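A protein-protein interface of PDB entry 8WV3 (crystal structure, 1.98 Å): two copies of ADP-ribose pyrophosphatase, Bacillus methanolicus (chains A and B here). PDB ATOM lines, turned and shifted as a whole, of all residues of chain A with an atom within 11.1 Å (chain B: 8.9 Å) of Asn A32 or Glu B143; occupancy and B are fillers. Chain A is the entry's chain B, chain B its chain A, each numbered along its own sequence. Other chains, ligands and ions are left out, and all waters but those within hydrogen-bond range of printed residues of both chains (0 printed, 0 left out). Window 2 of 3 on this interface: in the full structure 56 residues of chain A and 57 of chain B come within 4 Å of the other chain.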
ATOM      1  N   LYS A   3      -4.757  14.710  30.922  1.00  0.00           N
ATOM      2  CA  LYS A   3      -6.141  15.120  31.148  1.00  0.00           C
ATOM      3  C   LYS A   3      -6.546  16.273  30.230  1.00  0.00           C
ATOM      4  O   LYS A   3      -7.485  17.015  30.544  1.00  0.00           O
ATOM      5  CB  LYS A   3      -6.356  15.510  32.618  1.00  0.00           C
ATOM      6  CG  LYS A   3      -6.637  14.322  33.569  1.00  0.00           C
ATOM      7  CD  LYS A   3      -7.398  13.184  32.871  1.00  0.00           C
ATOM      8  CE  LYS A   3      -8.252  12.330  33.812  1.00  0.00           C
ATOM      9  NZ  LYS A   3      -9.676  12.771  33.904  1.00  0.00           N
ATOM     10  N   LEU A   4      -5.852  16.447  29.102  1.00  0.00           N
ATOM     11  CA  LEU A   4      -6.144  17.563  28.210  1.00  0.00           C
ATOM     12  C   LEU A   4      -7.582  17.492  27.693  1.00  0.00           C
ATOM     13  O   LEU A   4      -8.034  16.440  27.227  1.00  0.00           O
ATOM     14  CB  LEU A   4      -5.152  17.557  27.048  1.00  0.00           C
ATOM     15  CG  LEU A   4      -4.960  18.824  26.222  1.00  0.00           C
ATOM     16  CD1 LEU A   4      -4.462  19.963  27.092  1.00  0.00           C
ATOM     17  CD2 LEU A   4      -3.967  18.540  25.092  1.00  0.00           C
ATOM     18  N   PHE A   5      -8.306  18.626  27.775  1.00  0.00           N
ATOM     19  CA  PHE A   5      -9.686  18.735  27.267  1.00  0.00           C
ATOM     20  C   PHE A   5     -10.646  17.748  27.942  1.00  0.00           C
ATOM     21  O   PHE A   5     -11.593  17.256  27.320  1.00  0.00           O
ATOM     22  CB  PHE A   5      -9.763  18.549  25.746  1.00  0.00           C
ATOM     23  CG  PHE A   5      -8.676  19.257  24.972  1.00  0.00           C
ATOM     24  CD1 PHE A   5      -8.594  20.641  24.970  1.00  0.00           C
ATOM     25  CD2 PHE A   5      -7.759  18.536  24.223  1.00  0.00           C
ATOM     26  CE1 PHE A   5      -7.611  21.293  24.243  1.00  0.00           C
ATOM     27  CE2 PHE A   5      -6.769  19.180  23.500  1.00  0.00           C
ATOM     28  CZ  PHE A   5      -6.700  20.564  23.510  1.00  0.00           C
ATOM     29  N   GLU A   6     -10.435  17.492  29.226  1.00  0.00           N
ATOM     30  CA  GLU A   6     -11.253  16.524  29.949  1.00  0.00           C
ATOM     31  C   GLU A   6     -12.752  16.750  29.753  1.00  0.00           C
ATOM     32  O   GLU A   6     -13.246  17.880  29.785  1.00  0.00           O
ATOM     33  CB  GLU A   6     -10.904  16.563  31.436  1.00  0.00           C
ATOM     34  CG  GLU A   6     -11.681  15.520  32.254  1.00  0.00           C
ATOM     35  CD  GLU A   6     -11.214  15.445  33.690  1.00  0.00           C
ATOM     36  OE1 GLU A   6     -10.201  16.096  34.029  1.00  0.00           O
ATOM     37  OE2 GLU A   6     -11.877  14.745  34.481  1.00  0.00           O
ATOM     38  N   GLU A   7     -13.488  15.645  29.564  1.00  0.00           N
ATOM     39  CA  GLU A   7     -14.934  15.659  29.332  1.00  0.00           C
ATOM     40  C   GLU A   7     -15.650  15.008  30.522  1.00  0.00           C
ATOM     41  O   GLU A   7     -15.768  13.778  30.588  1.00  0.00           O
ATOM     42  CB  GLU A   7     -15.268  14.932  28.032  1.00  0.00           C
ATOM     43  CG  GLU A   7     -14.487  15.422  26.817  1.00  0.00           C
ATOM     44  CD  GLU A   7     -14.744  14.571  25.586  1.00  0.00           C
ATOM     45  OE1 GLU A   7     -15.135  13.388  25.738  1.00  0.00           O
ATOM     46  OE2 GLU A   7     -14.562  15.088  24.465  1.00  0.00           O
ATOM     47  N   LYS A   8     -16.169  15.833  31.434  1.00  0.00           N
ATOM     48  CA  LYS A   8     -16.769  15.313  32.661  1.00  0.00           C
ATOM     49  C   LYS A   8     -18.123  14.665  32.412  1.00  0.00           C
ATOM     50  O   LYS A   8     -18.977  15.206  31.703  1.00  0.00           O
ATOM     51  CB  LYS A   8     -16.915  16.425  33.711  1.00  0.00           C
ATOM     52  CG  LYS A   8     -15.599  16.864  34.349  1.00  0.00           C
ATOM     53  CD  LYS A   8     -15.072  18.186  33.801  1.00  0.00           C
ATOM     54  CE  LYS A   8     -14.015  18.780  34.730  1.00  0.00           C
ATOM     55  NZ  LYS A   8     -13.042  19.652  33.993  1.00  0.00           N
ATOM     56  N   VAL A  28     -21.679  14.195  28.589  1.00  0.00           N
ATOM     57  CA  VAL A  28     -20.433  14.770  29.070  1.00  0.00           C
ATOM     58  C   VAL A  28     -20.477  16.283  28.924  1.00  0.00           C
ATOM     59  O   VAL A  28     -21.213  16.835  28.102  1.00  0.00           O
ATOM     60  CB  VAL A  28     -19.194  14.193  28.336  1.00  0.00           C
ATOM     61  CG1 VAL A  28     -19.109  12.706  28.567  1.00  0.00           C
ATOM     62  CG2 VAL A  28     -19.243  14.517  26.833  1.00  0.00           C
ATOM     63  N   GLU A  29     -19.670  16.946  29.747  1.00  0.00           N
ATOM     64  CA  GLU A  29     -19.510  18.387  29.711  1.00  0.00           C
ATOM     65  C   GLU A  29     -18.171  18.677  29.039  1.00  0.00           C
ATOM     66  O   GLU A  29     -17.118  18.300  29.557  1.00  0.00           O
ATOM     67  CB  GLU A  29     -19.576  18.966  31.124  1.00  0.00           C
ATOM     68  CG  GLU A  29     -19.443  20.479  31.218  1.00  0.00           C
ATOM     69  CD  GLU A  29     -19.848  21.011  32.592  1.00  0.00           C
ATOM     70  OE1 GLU A  29     -19.041  20.900  33.544  1.00  0.00           O
ATOM     71  OE2 GLU A  29     -20.982  21.525  32.725  1.00  0.00           O
ATOM     72  N   LEU A  30     -18.215  19.320  27.882  1.00  0.00           N
ATOM     73  CA  LEU A  30     -17.003  19.680  27.165  1.00  0.00           C
ATOM     74  C   LEU A  30     -16.279  20.802  27.898  1.00  0.00           C
ATOM     75  O   LEU A  30     -16.840  21.445  28.786  1.00  0.00           O
ATOM     76  CB  LEU A  30     -17.344  20.100  25.737  1.00  0.00           C
ATOM     77  CG  LEU A  30     -18.085  19.019  24.962  1.00  0.00           C
ATOM     78  CD1 LEU A  30     -18.274  19.425  23.502  1.00  0.00           C
ATOM     79  CD2 LEU A  30     -17.283  17.729  25.073  1.00  0.00           C
ATOM     80  N   PRO A  31     -15.024  21.074  27.534  1.00  0.00           N
ATOM     81  CA  PRO A  31     -14.266  22.109  28.256  1.00  0.00           C
ATOM     82  C   PRO A  31     -14.910  23.488  28.197  1.00  0.00           C
ATOM     83  O   PRO A  31     -14.658  24.317  29.083  1.00  0.00           O
ATOM     84  CB  PRO A  31     -12.902  22.093  27.554  1.00  0.00           C
ATOM     85  CG  PRO A  31     -12.816  20.727  26.939  1.00  0.00           C
ATOM     86  CD  PRO A  31     -14.215  20.439  26.481  1.00  0.00           C
ATOM     87  N   ASN A  32     -15.743  23.754  27.193  1.00  0.00           N
ATOM     88  CA  ASN A  32     -16.326  25.072  26.985  1.00  0.00           C
ATOM     89  C   ASN A  32     -17.736  25.177  27.549  1.00  0.00           C
ATOM     90  O   ASN A  32     -18.454  26.130  27.226  1.00  0.00           O
ATOM     91  CB  ASN A  32     -16.327  25.414  25.492  1.00  0.00           C
ATOM     92  CG  ASN A  32     -17.153  24.441  24.672  1.00  0.00           C
ATOM     93  OD1 ASN A  32     -17.633  23.426  25.182  1.00  0.00           O
ATOM     94  ND2 ASN A  32     -17.314  24.739  23.393  1.00  0.00           N
ATOM     95  N   GLY A  33     -18.152  24.218  28.374  1.00  0.00           N
ATOM     96  CA  GLY A  33     -19.489  24.203  28.917  1.00  0.00           C
ATOM     97  C   GLY A  33     -20.546  23.569  28.034  1.00  0.00           C
ATOM     98  O   GLY A  33     -21.663  23.335  28.512  1.00  0.00           O
ATOM     99  N   GLN A  34     -20.247  23.291  26.765  1.00  0.00           N
ATOM    100  CA  GLN A  34     -21.190  22.548  25.941  1.00  0.00           C
ATOM    101  C   GLN A  34     -21.336  21.112  26.442  1.00  0.00           C
ATOM    102  O   GLN A  34     -20.528  20.608  27.228  1.00  0.00           O
ATOM    103  CB  GLN A  34     -20.748  22.534  24.482  1.00  0.00           C
ATOM    104  CG  GLN A  34     -21.047  23.810  23.757  1.00  0.00           C
ATOM    105  CD  GLN A  34     -22.230  24.507  24.370  1.00  0.00           C
ATOM    106  OE1 GLN A  34     -22.095  25.195  25.388  1.00  0.00           O
ATOM    107  NE2 GLN A  34     -23.414  24.304  23.784  1.00  0.00           N
ATOM    108  N   THR A  35     -22.381  20.447  25.958  1.00  0.00           N
ATOM    109  CA  THR A  35     -22.670  19.067  26.314  1.00  0.00           C
ATOM    110  C   THR A  35     -22.707  18.209  25.054  1.00  0.00           C
ATOM    111  O   THR A  35     -22.931  18.703  23.948  1.00  0.00           O
ATOM    112  CB  THR A  35     -24.003  18.945  27.066  1.00  0.00           C
ATOM    113  OG1 THR A  35     -25.029  19.610  26.318  1.00  0.00           O
ATOM    114  CG2 THR A  35     -23.892  19.589  28.446  1.00  0.00           C
ATOM    115  N   SER A  36     -22.472  16.912  25.232  1.00  0.00           N
ATOM    116  CA  SER A  36     -22.423  15.988  24.103  1.00  0.00           C
ATOM    117  C   SER A  36     -22.530  14.574  24.661  1.00  0.00           C
ATOM    118  O   SER A  36     -22.511  14.370  25.877  1.00  0.00           O
ATOM    119  CB  SER A  36     -21.142  16.183  23.282  1.00  0.00           C
ATOM    120  OG  SER A  36     -21.146  15.391  22.108  1.00  0.00           O
ATOM    121  N   ARG A  38     -21.283  10.403  24.597  1.00  0.00           N
ATOM    122  CA  ARG A  38     -20.139   9.524  24.384  1.00  0.00           C
ATOM    123  C   ARG A  38     -20.591   8.087  24.595  1.00  0.00           C
ATOM    124  O   ARG A  38     -21.049   7.727  25.687  1.00  0.00           O
ATOM    125  CB  ARG A  38     -18.977   9.855  25.330  1.00  0.00           C
ATOM    126  CG  ARG A  38     -18.366  11.230  25.101  1.00  0.00           C
ATOM    127  CD  ARG A  38     -17.505  11.259  23.859  1.00  0.00           C
ATOM    128  NE  ARG A  38     -16.919  12.583  23.659  1.00  0.00           N
ATOM    129  CZ  ARG A  38     -17.512  13.573  23.008  1.00  0.00           C
ATOM    130  NH1 ARG A  38     -18.696  13.413  22.443  1.00  0.00           N
ATOM    131  NH2 ARG A  38     -16.907  14.754  22.938  1.00  0.00           N
ATOM    132  N   GLU B  62      -3.145  15.249  19.998  1.00  0.00           N
ATOM    133  CA  GLU B  62      -3.594  14.899  21.341  1.00  0.00           C
ATOM    134  C   GLU B  62      -5.049  15.289  21.525  1.00  0.00           C
ATOM    135  O   GLU B  62      -5.471  16.378  21.117  1.00  0.00           O
ATOM    136  CB  GLU B  62      -2.746  15.557  22.431  1.00  0.00           C
ATOM    137  CG  GLU B  62      -3.112  15.001  23.817  1.00  0.00           C
ATOM    138  CD  GLU B  62      -2.093  15.264  24.924  1.00  0.00           C
ATOM    139  OE1 GLU B  62      -1.008  15.818  24.660  1.00  0.00           O
ATOM    140  OE2 GLU B  62      -2.414  14.929  26.091  1.00  0.00           O
ATOM    141  N   GLN B  63      -5.814  14.399  22.157  1.00  0.00           N
ATOM    142  CA  GLN B  63      -7.227  14.644  22.380  1.00  0.00           C
ATOM    143  C   GLN B  63      -7.687  13.748  23.525  1.00  0.00           C
ATOM    144  O   GLN B  63      -7.055  12.732  23.820  1.00  0.00           O
ATOM    145  CB  GLN B  63      -8.038  14.398  21.108  1.00  0.00           C
ATOM    146  CG  GLN B  63      -8.312  12.923  20.781  1.00  0.00           C
ATOM    147  CD  GLN B  63      -8.670  12.751  19.316  1.00  0.00           C
ATOM    148  OE1 GLN B  63      -7.863  12.272  18.519  1.00  0.00           O
ATOM    149  NE2 GLN B  63      -9.882  13.153  18.953  1.00  0.00           N
ATOM    150  N   GLU B  97      -7.467  17.432   9.891  1.00  0.00           N
ATOM    151  CA  GLU B  97      -7.055  17.350  11.288  1.00  0.00           C
ATOM    152  C   GLU B  97      -5.731  18.041  11.567  1.00  0.00           C
ATOM    153  O   GLU B  97      -5.471  18.419  12.716  1.00  0.00           O
ATOM    154  CB  GLU B  97      -6.955  15.881  11.714  1.00  0.00           C
ATOM    155  CG  GLU B  97      -8.073  15.419  12.621  1.00  0.00           C
ATOM    156  CD  GLU B  97      -7.860  13.998  13.089  1.00  0.00           C
ATOM    157  OE1 GLU B  97      -8.575  13.110  12.587  1.00  0.00           O
ATOM    158  OE2 GLU B  97      -6.978  13.765  13.935  1.00  0.00           O
ATOM    159  N   ASP B 142     -12.608  22.355  15.536  1.00  0.00           N
ATOM    160  CA  ASP B 142     -11.332  21.912  16.095  1.00  0.00           C
ATOM    161  C   ASP B 142     -11.313  22.066  17.624  1.00  0.00           C
ATOM    162  O   ASP B 142     -11.893  21.247  18.348  1.00  0.00           O
ATOM    163  CB  ASP B 142     -10.179  22.686  15.439  1.00  0.00           C
ATOM    164  CG  ASP B 142     -10.640  23.983  14.772  1.00  0.00           C
ATOM    165  OD1 ASP B 142     -11.411  23.907  13.789  1.00  0.00           O
ATOM    166  OD2 ASP B 142     -10.215  25.076  15.215  1.00  0.00           O
ATOM    167  N   GLU B 143     -10.625  23.101  18.110  1.00  0.00           N
ATOM    168  CA  GLU B 143     -10.691  23.493  19.516  1.00  0.00           C
ATOM    169  C   GLU B 143     -10.109  22.472  20.494  1.00  0.00           C
ATOM    170  O   GLU B 143      -9.230  22.813  21.295  1.00  0.00           O
ATOM    171  CB  GLU B 143     -12.139  23.789  19.909  1.00  0.00           C
ATOM    172  CG  GLU B 143     -12.292  25.066  20.695  1.00  0.00           C
ATOM    173  CD  GLU B 143     -13.743  25.439  20.927  1.00  0.00           C
ATOM    174  OE1 GLU B 143     -13.997  26.287  21.814  1.00  0.00           O
ATOM    175  OE2 GLU B 143     -14.625  24.888  20.222  1.00  0.00           O
ATOM    176  N   PHE B 144     -10.604  21.230  20.459  1.00  0.00           N
ATOM    177  CA  PHE B 144     -10.256  20.205  21.441  1.00  0.00           C
ATOM    178  C   PHE B 144      -9.329  19.133  20.873  1.00  0.00           C
ATOM    179  O   PHE B 144      -9.413  17.957  21.255  1.00  0.00           O
ATOM    180  CB  PHE B 144     -11.530  19.578  22.001  1.00  0.00           C
ATOM    181  CG  PHE B 144     -12.466  20.582  22.613  1.00  0.00           C
ATOM    182  CD1 PHE B 144     -11.990  21.528  23.509  1.00  0.00           C
ATOM    183  CD2 PHE B 144     -13.801  20.615  22.261  1.00  0.00           C
ATOM    184  CE1 PHE B 144     -12.842  22.470  24.067  1.00  0.00           C
ATOM    185  CE2 PHE B 144     -14.652  21.549  22.816  1.00  0.00           C
ATOM    186  CZ  PHE B 144     -14.172  22.478  23.720  1.00  0.00           C
ATOM    187  N   VAL B 145      -8.448  19.531  19.956  1.00  0.00           N
ATOM    188  CA  VAL B 145      -7.394  18.675  19.422  1.00  0.00           C
ATOM    189  C   VAL B 145      -6.124  19.505  19.358  1.00  0.00           C
ATOM    190  O   VAL B 145      -6.132  20.603  18.793  1.00  0.00           O
ATOM    191  CB  VAL B 145      -7.738  18.124  18.024  1.00  0.00           C
ATOM    192  CG1 VAL B 145      -6.532  17.372  17.428  1.00  0.00           C
ATOM    193  CG2 VAL B 145      -8.957  17.243  18.085  1.00  0.00           C
ATOM    194  N   ASP B 146      -5.044  18.996  19.948  1.00  0.00           N
ATOM    195  CA  ASP B 146      -3.737  19.647  19.934  1.00  0.00           C
ATOM    196  C   ASP B 146      -2.852  18.987  18.879  1.00  0.00           C
ATOM    197  O   ASP B 146      -2.680  17.766  18.892  1.00  0.00           O
ATOM    198  CB  ASP B 146      -3.078  19.540  21.309  1.00  0.00           C
ATOM    199  CG  ASP B 146      -2.009  20.594  21.545  1.00  0.00           C
ATOM    200  OD1 ASP B 146      -1.562  21.265  20.582  1.00  0.00           O
ATOM    201  OD2 ASP B 146      -1.581  20.722  22.712  1.00  0.00           O
ATOM    202  N   LEU B 147      -2.307  19.787  17.966  1.00  0.00           N
ATOM    203  CA  LEU B 147      -1.353  19.292  16.981  1.00  0.00           C
ATOM    204  C   LEU B 147       0.019  19.171  17.617  1.00  0.00           C
ATOM    205  O   LEU B 147       0.456  20.060  18.351  1.00  0.00           O
ATOM    206  CB  LEU B 147      -1.286  20.229  15.769  1.00  0.00           C
ATOM    207  CG  LEU B 147      -0.576  19.657  14.543  1.00  0.00           C
ATOM    208  CD1 LEU B 147      -1.303  18.405  14.077  1.00  0.00           C
ATOM    209  CD2 LEU B 147      -0.489  20.694  13.397  1.00  0.00           C
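The backbone NH (N) of Glu B62 lies within hydrogen-bond range of the backbone carbonyl oxygen (O) of Asp B146 (2.8 Å).
The backbone NH (N) of Gln A34 is in hydrogen-bond range of the side-chain amide oxygen (OD1) of Asn A32.
Among the printed residues, merely in contact across the chains: Pro A31 with Phe B144, Phe A5 with Phe B144, Phe A5 with Glu B143, Asn A32 with Phe B144, Leu A4 with Glu B62, Phe A5 with Glu B62, Phe A5 with Val B145, Phe A5 with Asp B146 and Asn A32 with Glu B143.
Of the printed residues of chain A, Glu B143 touches Phe A5 (3.7 Å) and Asn A32 (3.99 Å).
Pro A31 touches one residue of chain B.
No residue of chain B comes within 4 Å of Gly A33.
No residue of chain A comes within 4 Å of Asp B142.
Of the printed residues of chain A, Phe B144 touches Phe A5, Pro A31 and Asn A32.
Val B145 touches just one residue of chain A: Phe A5 (3.9 Å).
Of the printed residues of chain A, Asp B146 touches Phe A5.
Of the printed residues of chain B, Leu A4 touches Glu B62 (3.8 Å).
Of the printed residues of chain B, Phe A5 touches Glu B62 (3.9 Å), Glu B143 (3.7 Å), Phe B144 (3.4 Å), Val B145 (3.9 Å) and Asp B146 (3.95 Å).
Printed residues of chain A within 4 Å of Glu B62: Leu A4 (3.8 Å) and Phe A5 (3.9 Å).
Glu B97 touches none of the printed residues of chain A.
The nearest printed residue of chain B that does not touch Asn A32 is Asp B142 (8.2 Å).
The nearest printed residue of chain B that does not touch Leu A4 is Asp B146 (4.01 Å).
No position is printed for both chains.
Of the 9 pairs that touch across the chains among the printed residues, none has its exchanged pair printed and touching as well.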
